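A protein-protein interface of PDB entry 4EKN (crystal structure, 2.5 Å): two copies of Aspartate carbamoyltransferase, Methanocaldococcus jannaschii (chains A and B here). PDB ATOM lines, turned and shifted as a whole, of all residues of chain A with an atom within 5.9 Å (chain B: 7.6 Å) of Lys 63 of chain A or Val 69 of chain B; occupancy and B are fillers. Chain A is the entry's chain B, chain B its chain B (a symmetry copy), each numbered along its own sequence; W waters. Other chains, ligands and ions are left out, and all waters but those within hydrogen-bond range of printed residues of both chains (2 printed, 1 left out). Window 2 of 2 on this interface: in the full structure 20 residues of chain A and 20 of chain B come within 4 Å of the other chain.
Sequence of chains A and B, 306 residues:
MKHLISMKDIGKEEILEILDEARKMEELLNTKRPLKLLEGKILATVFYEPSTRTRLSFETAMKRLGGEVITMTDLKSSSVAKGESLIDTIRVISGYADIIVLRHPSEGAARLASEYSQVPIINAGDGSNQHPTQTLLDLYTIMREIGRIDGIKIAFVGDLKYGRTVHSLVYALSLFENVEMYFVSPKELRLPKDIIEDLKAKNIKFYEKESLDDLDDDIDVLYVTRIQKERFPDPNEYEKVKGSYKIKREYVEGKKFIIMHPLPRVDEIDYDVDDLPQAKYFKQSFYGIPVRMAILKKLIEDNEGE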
ATOM      1  N   LEU A  35     -23.448  20.831   0.665  1.00  0.00           N
ATOM      2  CA  LEU A  35     -24.430  21.335   1.616  1.00  0.00           C
ATOM      3  C   LEU A  35     -23.875  21.277   3.033  1.00  0.00           C
ATOM      4  O   LEU A  35     -23.228  20.301   3.409  1.00  0.00           O
ATOM      5  CB  LEU A  35     -25.711  20.507   1.538  1.00  0.00           C
ATOM      6  CG  LEU A  35     -26.295  20.240   0.152  1.00  0.00           C
ATOM      7  CD1 LEU A  35     -27.509  19.332   0.268  1.00  0.00           C
ATOM      8  CD2 LEU A  35     -26.657  21.542  -0.550  1.00  0.00           C
ATOM      9  N   PHE A  58     -29.291   6.341   5.790  1.00  0.00           N
ATOM     10  CA  PHE A  58     -29.191   7.384   6.800  1.00  0.00           C
ATOM     11  C   PHE A  58     -27.797   8.004   6.818  1.00  0.00           C
ATOM     12  O   PHE A  58     -27.645   9.216   6.960  1.00  0.00           O
ATOM     13  CB  PHE A  58     -29.533   6.834   8.181  1.00  0.00           C
ATOM     14  CG  PHE A  58     -31.003   6.791   8.467  1.00  0.00           C
ATOM     15  CD1 PHE A  58     -31.696   7.954   8.759  1.00  0.00           C
ATOM     16  CD2 PHE A  58     -31.690   5.591   8.460  1.00  0.00           C
ATOM     17  CE1 PHE A  58     -33.049   7.921   9.031  1.00  0.00           C
ATOM     18  CE2 PHE A  58     -33.044   5.551   8.733  1.00  0.00           C
ATOM     19  CZ  PHE A  58     -33.724   6.717   9.020  1.00  0.00           C
ATOM     20  N   GLU A  59     -26.781   7.164   6.668  1.00  0.00           N
ATOM     21  CA  GLU A  59     -25.408   7.634   6.673  1.00  0.00           C
ATOM     22  C   GLU A  59     -25.166   8.553   5.474  1.00  0.00           C
ATOM     23  O   GLU A  59     -24.510   9.590   5.590  1.00  0.00           O
ATOM     24  CB  GLU A  59     -24.442   6.446   6.661  1.00  0.00           C
ATOM     25  CG  GLU A  59     -23.005   6.812   6.983  1.00  0.00           C
ATOM     26  CD  GLU A  59     -22.099   5.601   7.079  1.00  0.00           C
ATOM     27  OE1 GLU A  59     -22.464   4.631   7.780  1.00  0.00           O
ATOM     28  OE2 GLU A  59     -21.022   5.617   6.449  1.00  0.00           O
ATOM     29  N   THR A  60     -25.712   8.167   4.324  1.00  0.00           N
ATOM     30  CA  THR A  60     -25.648   8.999   3.127  1.00  0.00           C
ATOM     31  C   THR A  60     -26.388  10.316   3.346  1.00  0.00           C
ATOM     32  O   THR A  60     -25.866  11.390   3.055  1.00  0.00           O
ATOM     33  CB  THR A  60     -26.268   8.289   1.916  1.00  0.00           C
ATOM     34  OG1 THR A  60     -25.582   7.054   1.679  1.00  0.00           O
ATOM     35  CG2 THR A  60     -26.176   9.168   0.683  1.00  0.00           C
ATOM     36  N   ALA A  61     -27.608  10.223   3.863  1.00  0.00           N
ATOM     37  CA  ALA A  61     -28.418  11.402   4.138  1.00  0.00           C
ATOM     38  C   ALA A  61     -27.682  12.392   5.036  1.00  0.00           C
ATOM     39  O   ALA A  61     -27.610  13.584   4.731  1.00  0.00           O
ATOM     40  CB  ALA A  61     -29.743  10.999   4.765  1.00  0.00           C
ATOM     41  N   MET A  62     -27.126  11.895   6.136  1.00  0.00           N
ATOM     42  CA  MET A  62     -26.405  12.751   7.075  1.00  0.00           C
ATOM     43  C   MET A  62     -25.170  13.381   6.442  1.00  0.00           C
ATOM     44  O   MET A  62     -24.878  14.557   6.654  1.00  0.00           O
ATOM     45  CB  MET A  62     -26.001  11.965   8.319  1.00  0.00           C
ATOM     46  CG  MET A  62     -25.447  12.830   9.429  1.00  0.00           C
ATOM     47  SD  MET A  62     -26.632  14.083   9.938  1.00  0.00           S
ATOM     48  CE  MET A  62     -25.817  14.763  11.383  1.00  0.00           C
ATOM     49  N   LYS A  63     -24.440  12.594   5.663  1.00  0.00           N
ATOM     50  CA  LYS A  63     -23.233  13.100   5.021  1.00  0.00           C
ATOM     51  C   LYS A  63     -23.530  14.087   3.895  1.00  0.00           C
ATOM     52  O   LYS A  63     -22.746  15.005   3.650  1.00  0.00           O
ATOM     53  CB  LYS A  63     -22.343  11.946   4.555  1.00  0.00           C
ATOM     54  CG  LYS A  63     -21.581  11.302   5.711  1.00  0.00           C
ATOM     55  CD  LYS A  63     -21.066   9.914   5.377  1.00  0.00           C
ATOM     56  CE  LYS A  63     -20.287   9.344   6.552  1.00  0.00           C
ATOM     57  NZ  LYS A  63     -19.765   7.985   6.270  1.00  0.00           N
ATOM     58  N   ARG A  64     -24.669  13.911   3.226  1.00  0.00           N
ATOM     59  CA  ARG A  64     -25.099  14.853   2.196  1.00  0.00           C
ATOM     60  C   ARG A  64     -25.405  16.211   2.817  1.00  0.00           C
ATOM     61  O   ARG A  64     -25.358  17.241   2.143  1.00  0.00           O
ATOM     62  CB  ARG A  64     -26.334  14.340   1.453  1.00  0.00           C
ATOM     63  CG  ARG A  64     -26.065  13.224   0.460  1.00  0.00           C
ATOM     64  CD  ARG A  64     -25.116  13.663  -0.648  1.00  0.00           C
ATOM     65  NE  ARG A  64     -25.018  12.656  -1.703  1.00  0.00           N
ATOM     66  CZ  ARG A  64     -24.084  12.643  -2.647  1.00  0.00           C
ATOM     67  NH1 ARG A  64     -23.149  13.586  -2.675  1.00  0.00           N
ATOM     68  NH2 ARG A  64     -24.082  11.682  -3.563  1.00  0.00           N
ATOM     69  N   LEU A  65     -25.741  16.204   4.103  1.00  0.00           N
ATOM     70  CA  LEU A  65     -26.062  17.435   4.818  1.00  0.00           C
ATOM     71  C   LEU A  65     -24.824  18.011   5.490  1.00  0.00           C
ATOM     72  O   LEU A  65     -24.921  18.919   6.310  1.00  0.00           O
ATOM     73  CB  LEU A  65     -27.155  17.187   5.858  1.00  0.00           C
ATOM     74  CG  LEU A  65     -28.571  17.001   5.306  1.00  0.00           C
ATOM     75  CD1 LEU A  65     -29.524  16.557   6.402  1.00  0.00           C
ATOM     76  CD2 LEU A  65     -29.063  18.282   4.640  1.00  0.00           C
ATOM     77  N   GLY A  66     -23.661  17.471   5.139  1.00  0.00           N
ATOM     78  CA  GLY A  66     -22.403  17.944   5.680  1.00  0.00           C
ATOM     79  C   GLY A  66     -22.145  17.484   7.102  1.00  0.00           C
ATOM     80  O   GLY A  66     -21.215  17.955   7.756  1.00  0.00           O
ATOM     81  N   GLY A  67     -22.965  16.558   7.583  1.00  0.00           N
ATOM     82  CA  GLY A  67     -22.836  16.069   8.942  1.00  0.00           C
ATOM     83  C   GLY A  67     -21.892  14.889   9.059  1.00  0.00           C
ATOM     84  O   GLY A  67     -21.369  14.399   8.062  1.00  0.00           O
ATOM     85  N   GLU A  68     -21.678  14.437  10.291  1.00  0.00           N
ATOM     86  CA  GLU A  68     -20.821  13.289  10.559  1.00  0.00           C
ATOM     87  C   GLU A  68     -21.636  12.094  11.051  1.00  0.00           C
ATOM     88  O   GLU A  68     -22.797  12.239  11.436  1.00  0.00           O
ATOM     89  CB  GLU A  68     -19.744  13.651  11.584  1.00  0.00           C
ATOM     90  CG  GLU A  68     -18.753  14.692  11.096  1.00  0.00           C
ATOM     91  CD  GLU A  68     -18.000  14.234   9.863  1.00  0.00           C
ATOM     92  OE1 GLU A  68     -17.396  15.090   9.182  1.00  0.00           O
ATOM     93  OE2 GLU A  68     -18.014  13.018   9.578  1.00  0.00           O
ATOM     94  N   VAL A  69     -21.024  10.915  11.039  1.00  0.00           N
ATOM     95  CA  VAL A  69     -21.712   9.701  11.465  1.00  0.00           C
ATOM     96  C   VAL A  69     -20.796   8.753  12.227  1.00  0.00           C
ATOM     97  O   VAL A  69     -19.701   8.431  11.763  1.00  0.00           O
ATOM     98  CB  VAL A  69     -22.293   8.927  10.256  1.00  0.00           C
ATOM     99  CG1 VAL A  69     -22.882   7.605  10.710  1.00  0.00           C
ATOM    100  CG2 VAL A  69     -23.338   9.764   9.525  1.00  0.00           C
ATOM    101  N   GLY B  40     -18.139  17.383  -0.606  1.00  0.00           N
ATOM    102  CA  GLY B  40     -19.522  17.173  -0.992  1.00  0.00           C
ATOM    103  C   GLY B  40     -19.727  15.935  -1.843  1.00  0.00           C
ATOM    104  O   GLY B  40     -20.852  15.622  -2.239  1.00  0.00           O
ATOM    105  N   LYS B  41     -18.640  15.227  -2.129  1.00  0.00           N
ATOM    106  CA  LYS B  41     -18.718  14.006  -2.927  1.00  0.00           C
ATOM    107  C   LYS B  41     -18.615  12.761  -2.049  1.00  0.00           C
ATOM    108  O   LYS B  41     -17.876  12.739  -1.062  1.00  0.00           O
ATOM    109  CB  LYS B  41     -17.631  13.987  -4.001  1.00  0.00           C
ATOM    110  CG  LYS B  41     -17.686  15.160  -4.969  1.00  0.00           C
ATOM    111  CD  LYS B  41     -18.972  15.161  -5.781  1.00  0.00           C
ATOM    112  CE  LYS B  41     -18.942  16.242  -6.855  1.00  0.00           C
ATOM    113  NZ  LYS B  41     -20.162  16.229  -7.699  1.00  0.00           N
ATOM    114  N   ILE B  42     -19.354  11.722  -2.420  1.00  0.00           N
ATOM    115  CA  ILE B  42     -19.394  10.497  -1.636  1.00  0.00           C
ATOM    116  C   ILE B  42     -18.832   9.283  -2.373  1.00  0.00           C
ATOM    117  O   ILE B  42     -19.296   8.928  -3.458  1.00  0.00           O
ATOM    118  CB  ILE B  42     -20.828  10.182  -1.166  1.00  0.00           C
ATOM    119  CG1 ILE B  42     -21.345  11.310  -0.266  1.00  0.00           C
ATOM    120  CG2 ILE B  42     -20.864   8.844  -0.442  1.00  0.00           C
ATOM    121  CD1 ILE B  42     -22.664  11.008   0.425  1.00  0.00           C
ATOM    122  N   LEU B  43     -17.834   8.644  -1.768  1.00  0.00           N
ATOM    123  CA  LEU B  43     -17.294   7.392  -2.282  1.00  0.00           C
ATOM    124  C   LEU B  43     -17.959   6.207  -1.601  1.00  0.00           C
ATOM    125  O   LEU B  43     -18.039   6.148  -0.378  1.00  0.00           O
ATOM    126  CB  LEU B  43     -15.785   7.314  -2.058  1.00  0.00           C
ATOM    127  CG  LEU B  43     -15.218   5.899  -2.224  1.00  0.00           C
ATOM    128  CD1 LEU B  43     -15.402   5.410  -3.659  1.00  0.00           C
ATOM    129  CD2 LEU B  43     -13.755   5.838  -1.817  1.00  0.00           C
ATOM    130  N   ALA B  44     -18.437   5.258  -2.397  1.00  0.00           N
ATOM    131  CA  ALA B  44     -19.034   4.051  -1.847  1.00  0.00           C
ATOM    132  C   ALA B  44     -18.101   2.864  -2.025  1.00  0.00           C
ATOM    133  O   ALA B  44     -17.760   2.488  -3.150  1.00  0.00           O
ATOM    134  CB  ALA B  44     -20.384   3.776  -2.496  1.00  0.00           C
ATOM    135  N   THR B  45     -17.676   2.292  -0.906  1.00  0.00           N
ATOM    136  CA  THR B  45     -16.844   1.094  -0.908  1.00  0.00           C
ATOM    137  C   THR B  45     -17.727  -0.150  -0.901  1.00  0.00           C
ATOM    138  O   THR B  45     -18.420  -0.435   0.079  1.00  0.00           O
ATOM    139  CB  THR B  45     -15.869   1.083   0.293  1.00  0.00           C
ATOM    140  OG1 THR B  45     -14.556   1.441  -0.157  1.00  0.00           O
ATOM    141  CG2 THR B  45     -15.813  -0.287   0.943  1.00  0.00           C
ATOM    142  N   ARG B  55      -9.753  -1.013   1.195  1.00  0.00           N
ATOM    143  CA  ARG B  55     -10.707  -0.075   1.767  1.00  0.00           C
ATOM    144  C   ARG B  55     -10.018   1.120   2.426  1.00  0.00           C
ATOM    145  O   ARG B  55     -10.383   2.268   2.173  1.00  0.00           O
ATOM    146  CB  ARG B  55     -11.625  -0.772   2.773  1.00  0.00           C
ATOM    147  CG  ARG B  55     -12.719   0.138   3.313  1.00  0.00           C
ATOM    148  CD  ARG B  55     -13.564  -0.555   4.359  1.00  0.00           C
ATOM    149  NE  ARG B  55     -12.768  -0.949   5.516  1.00  0.00           N
ATOM    150  CZ  ARG B  55     -12.533  -0.168   6.564  1.00  0.00           C
ATOM    151  NH1 ARG B  55     -13.032   1.061   6.609  1.00  0.00           N
ATOM    152  NH2 ARG B  55     -11.798  -0.617   7.572  1.00  0.00           N
ATOM    153  N   PHE B  58      -8.250   3.699  -0.227  1.00  0.00           N
ATOM    154  CA  PHE B  58      -9.241   4.484  -0.946  1.00  0.00           C
ATOM    155  C   PHE B  58      -9.983   5.432  -0.009  1.00  0.00           C
ATOM    156  O   PHE B  58     -10.258   6.580  -0.356  1.00  0.00           O
ATOM    157  CB  PHE B  58     -10.236   3.576  -1.661  1.00  0.00           C
ATOM    158  CG  PHE B  58      -9.758   3.083  -2.992  1.00  0.00           C
ATOM    159  CD1 PHE B  58      -9.743   3.927  -4.090  1.00  0.00           C
ATOM    160  CD2 PHE B  58      -9.338   1.775  -3.153  1.00  0.00           C
ATOM    161  CE1 PHE B  58      -9.309   3.478  -5.321  1.00  0.00           C
ATOM    162  CE2 PHE B  58      -8.904   1.319  -4.384  1.00  0.00           C
ATOM    163  CZ  PHE B  58      -8.891   2.171  -5.469  1.00  0.00           C
ATOM    164  N   GLU B  59     -10.301   4.946   1.184  1.00  0.00           N
ATOM    165  CA  GLU B  59     -11.012   5.750   2.160  1.00  0.00           C
ATOM    166  C   GLU B  59     -10.148   6.939   2.585  1.00  0.00           C
ATOM    167  O   GLU B  59     -10.637   8.061   2.727  1.00  0.00           O
ATOM    168  CB  GLU B  59     -11.402   4.893   3.367  1.00  0.00           C
ATOM    169  CG  GLU B  59     -12.414   5.547   4.291  1.00  0.00           C
ATOM    170  CD  GLU B  59     -12.867   4.629   5.408  1.00  0.00           C
ATOM    171  OE1 GLU B  59     -13.235   3.468   5.121  1.00  0.00           O
ATOM    172  OE2 GLU B  59     -12.853   5.067   6.576  1.00  0.00           O
ATOM    173  N   THR B  60      -8.858   6.684   2.776  1.00  0.00           N
ATOM    174  CA  THR B  60      -7.902   7.744   3.082  1.00  0.00           C
ATOM    175  C   THR B  60      -7.810   8.736   1.927  1.00  0.00           C
ATOM    176  O   THR B  60      -7.883   9.947   2.126  1.00  0.00           O
ATOM    177  CB  THR B  60      -6.501   7.177   3.350  1.00  0.00           C
ATOM    178  OG1 THR B  60      -6.555   6.251   4.441  1.00  0.00           O
ATOM    179  CG2 THR B  60      -5.532   8.297   3.678  1.00  0.00           C
ATOM    180  N   ALA B  61      -7.652   8.212   0.717  1.00  0.00           N
ATOM    181  CA  ALA B  61      -7.565   9.044  -0.476  1.00  0.00           C
ATOM    182  C   ALA B  61      -8.769   9.974  -0.601  1.00  0.00           C
ATOM    183  O   ALA B  61      -8.616  11.178  -0.809  1.00  0.00           O
ATOM    184  CB  ALA B  61      -7.431   8.178  -1.717  1.00  0.00           C
ATOM    185  N   MET B  62      -9.967   9.414  -0.464  1.00  0.00           N
ATOM    186  CA  MET B  62     -11.191  10.203  -0.574  1.00  0.00           C
ATOM    187  C   MET B  62     -11.290  11.261   0.519  1.00  0.00           C
ATOM    188  O   MET B  62     -11.692  12.396   0.269  1.00  0.00           O
ATOM    189  CB  MET B  62     -12.419   9.300  -0.529  1.00  0.00           C
ATOM    190  CG  MET B  62     -13.711  10.016  -0.858  1.00  0.00           C
ATOM    191  SD  MET B  62     -13.648  10.768  -2.490  1.00  0.00           S
ATOM    192  CE  MET B  62     -15.346  11.306  -2.689  1.00  0.00           C
ATOM    193  N   LYS B  63     -10.924  10.886   1.737  1.00  0.00           N
ATOM    194  CA  LYS B  63     -10.994  11.821   2.853  1.00  0.00           C
ATOM    195  C   LYS B  63      -9.932  12.915   2.775  1.00  0.00           C
ATOM    196  O   LYS B  63     -10.164  14.038   3.224  1.00  0.00           O
ATOM    197  CB  LYS B  63     -10.955  11.075   4.189  1.00  0.00           C
ATOM    198  CG  LYS B  63     -12.294  10.420   4.523  1.00  0.00           C
ATOM    199  CD  LYS B  63     -12.171   9.325   5.566  1.00  0.00           C
ATOM    200  CE  LYS B  63     -13.539   8.740   5.880  1.00  0.00           C
ATOM    201  NZ  LYS B  63     -13.465   7.664   6.898  1.00  0.00           N
ATOM    202  N   GLY B  67     -13.567  14.579   0.763  1.00  0.00           N
ATOM    203  CA  GLY B  67     -14.779  13.857   0.430  1.00  0.00           C
ATOM    204  C   GLY B  67     -15.272  12.974   1.558  1.00  0.00           C
ATOM    205  O   GLY B  67     -14.633  12.870   2.603  1.00  0.00           O
ATOM    206  N   GLU B  68     -16.418  12.337   1.339  1.00  0.00           N
ATOM    207  CA  GLU B  68     -17.000  11.427   2.318  1.00  0.00           C
ATOM    208  C   GLU B  68     -16.951   9.982   1.826  1.00  0.00           C
ATOM    209  O   GLU B  68     -16.721   9.725   0.643  1.00  0.00           O
ATOM    210  CB  GLU B  68     -18.443  11.828   2.630  1.00  0.00           C
ATOM    211  CG  GLU B  68     -18.574  13.175   3.317  1.00  0.00           C
ATOM    212  CD  GLU B  68     -17.847  13.215   4.646  1.00  0.00           C
ATOM    213  OE1 GLU B  68     -17.607  14.327   5.161  1.00  0.00           O
ATOM    214  OE2 GLU B  68     -17.515  12.131   5.172  1.00  0.00           O
ATOM    215  N   VAL B  69     -17.168   9.039   2.737  1.00  0.00           N
ATOM    216  CA  VAL B  69     -17.123   7.623   2.387  1.00  0.00           C
ATOM    217  C   VAL B  69     -18.175   6.809   3.127  1.00  0.00           C
ATOM    218  O   VAL B  69     -18.292   6.899   4.350  1.00  0.00           O
ATOM    219  CB  VAL B  69     -15.738   7.007   2.706  1.00  0.00           C
ATOM    220  CG1 VAL B  69     -15.758   5.510   2.463  1.00  0.00           C
ATOM    221  CG2 VAL B  69     -14.641   7.675   1.883  1.00  0.00           C
ATOM    222  N   ILE B  70     -18.941   6.018   2.380  1.00  0.00           N
ATOM    223  CA  ILE B  70     -19.811   5.006   2.974  1.00  0.00           C
ATOM    224  C   ILE B  70     -19.260   3.624   2.636  1.00  0.00           C
ATOM    225  O   ILE B  70     -18.714   3.419   1.553  1.00  0.00           O
ATOM    226  CB  ILE B  70     -21.274   5.123   2.495  1.00  0.00           C
ATOM    227  CG1 ILE B  70     -21.366   4.896   0.984  1.00  0.00           C
ATOM    228  CG2 ILE B  70     -21.861   6.476   2.879  1.00  0.00           C
ATOM    229  CD1 ILE B  70     -22.780   4.945   0.449  1.00  0.00           C
ATOM    230  N   THR B  71     -19.410   2.679   3.559  1.00  0.00           N
ATOM    231  CA  THR B  71     -18.737   1.387   3.445  1.00  0.00           C
ATOM    232  C   THR B  71     -19.685   0.187   3.463  1.00  0.00           C
ATOM    233  O   THR B  71     -20.625   0.130   4.253  1.00  0.00           O
ATOM    234  CB  THR B  71     -17.684   1.221   4.557  1.00  0.00           C
ATOM    235  OG1 THR B  71     -16.608   2.144   4.337  1.00  0.00           O
ATOM    236  CG2 THR B  71     -17.135  -0.191   4.562  1.00  0.00           C
ATOM    237  N   MET B  72     -19.416  -0.775   2.588  1.00  0.00           N
ATOM    238  CA  MET B  72     -20.216  -1.990   2.478  1.00  0.00           C
ATOM    239  C   MET B  72     -19.267  -3.142   2.161  1.00  0.00           C
ATOM    240  O   MET B  72     -18.972  -3.403   0.995  1.00  0.00           O
ATOM    241  CB  MET B  72     -21.245  -1.826   1.360  1.00  0.00           C
ATOM    242  CG  MET B  72     -22.390  -2.821   1.382  1.00  0.00           C
ATOM    243  SD  MET B  72     -23.535  -2.516   0.020  1.00  0.00           S
ATOM    244  CE  MET B  72     -24.959  -3.475   0.529  1.00  0.00           C
ATOM    245  N   LEU B 296      -9.565   8.950  -8.080  1.00  0.00           N
ATOM    246  CA  LEU B 296     -10.857   9.402  -7.578  1.00  0.00           C
ATOM    247  C   LEU B 296     -11.252  10.725  -8.215  1.00  0.00           C
ATOM    248  O   LEU B 296     -12.333  10.849  -8.784  1.00  0.00           O
ATOM    249  CB  LEU B 296     -10.828   9.545  -6.057  1.00  0.00           C
ATOM    250  CG  LEU B 296     -10.825   8.245  -5.243  1.00  0.00           C
ATOM    251  CD1 LEU B 296     -10.591   8.531  -3.763  1.00  0.00           C
ATOM    252  CD2 LEU B 296     -12.122   7.476  -5.450  1.00  0.00           C
HETATM  253  O   HOH W   1     -17.191   9.753   5.920  1.00  0.00           O
HETATM  254  O   HOH W   2     -19.463   3.614   5.997  1.00  0.00           O
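The side-chain amino group of Lys 63 of chain A sits at hydrogen-bond distance from the backbone carbonyl oxygen of Val 69 of chain B, 2.7 Å away.
The backbone carbonyl oxygen (O) of Gly 40 of chain B lies within hydrogen-bond range of the guanidinium group (NH1) of Arg 64 of chain A, 3.1 Å away.
The backbone NH of Ile 70 of chain B sits at hydrogen-bond distance from the backbone carbonyl oxygen of Leu 43 of chain B (2.9 Å).
The side-chain carboxylate (OE2) of Glu 59 of chain A is in salt-bridge range of the side-chain amino group (NZ) of Lys 63 of chain A (2.7 Å).
O of Ile 70 of chain B lies within hydrogen-bond range of N of Thr 45 of chain B, 2.9 Å away.
Among the printed residues, merely in contact across the chains: Glu 59 of chain A with Val 69 of chain B (3.7 Å), Glu 59 of chain A with Ile 70 of chain B (3.7 Å), Thr 60 of chain A with Ile 42 of chain B (3.97 Å), Thr 60 of chain A with Ile 70 of chain B (3.7 Å) and Arg 64 of chain A with Ile 42 of chain B (3.6 Å).
Leu 35 of chain A touches none of the printed residues of chain B.
Printed residues of chain B within 4 Å of Glu 59 of chain A: Val 69 and Ile 70.
Printed residues of chain B within 4 Å of Thr 60 of chain A: Ile 42 and Ile 70.
Printed residues of chain B within 4 Å of Arg 64 of chain A: Gly 40 and Ile 42.
Val 69 of chain A touches none of the printed residues of chain B.
Of the printed residues of chain A, Gly 40 of chain B touches Arg 64 (3.1 Å).
Of the printed residues of chain A, Ile 42 of chain B touches Thr 60 (3.97 Å) and Arg 64 (3.6 Å).
Val 69 of chain B touches just these residues of chain A: Glu 59 (3.7 Å) and Lys 63 (2.7 Å).
Printed residues of chain A that touch a printed residue of chain B: Glu 59, Thr 60, Lys 63 and Arg 64.
Of the 20 printed residues of chain B, 4 touch a printed residue of chain A.
Hydrophobic or aromatic side chains of chain B within 4 Å of the printed part of chain A: Ile 42 and Ile 70.
Along chain B the printed residues that touch a printed residue of chain A span positions 40 to 70.
Among the printed residues, no Asp or Glu carboxylate lies within 4 Å of a Lys or Arg side-chain nitrogen of the other chain.
Glu 59 of chain A touches Val 69 of chain B, but with the chains exchanged Val 69 of chain A does not touch Glu 59 of chain B (9.2 Å).
Lys 63 of chain A touches Val 69 of chain B, but with the chains exchanged Val 69 of chain A does not touch Lys 63 of chain B (7.9 Å).
9 positions are printed for both chains.
Of the 7 pairs that touch across the chains among the printed residues, none has its exchanged pair printed and touching as well.
Water W1 lies within hydrogen-bond range of the side-chain carboxylate of Glu 68 of chain B, the side-chain amino group of Lys 63 of chain A and the backbone NH of Val 69 of chain B.
Water W2 bridges the side-chain carboxylate of Glu 59 of chain A (2.6 Å) and the backbone NH of Thr 71 of chain B (2.6 Å).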
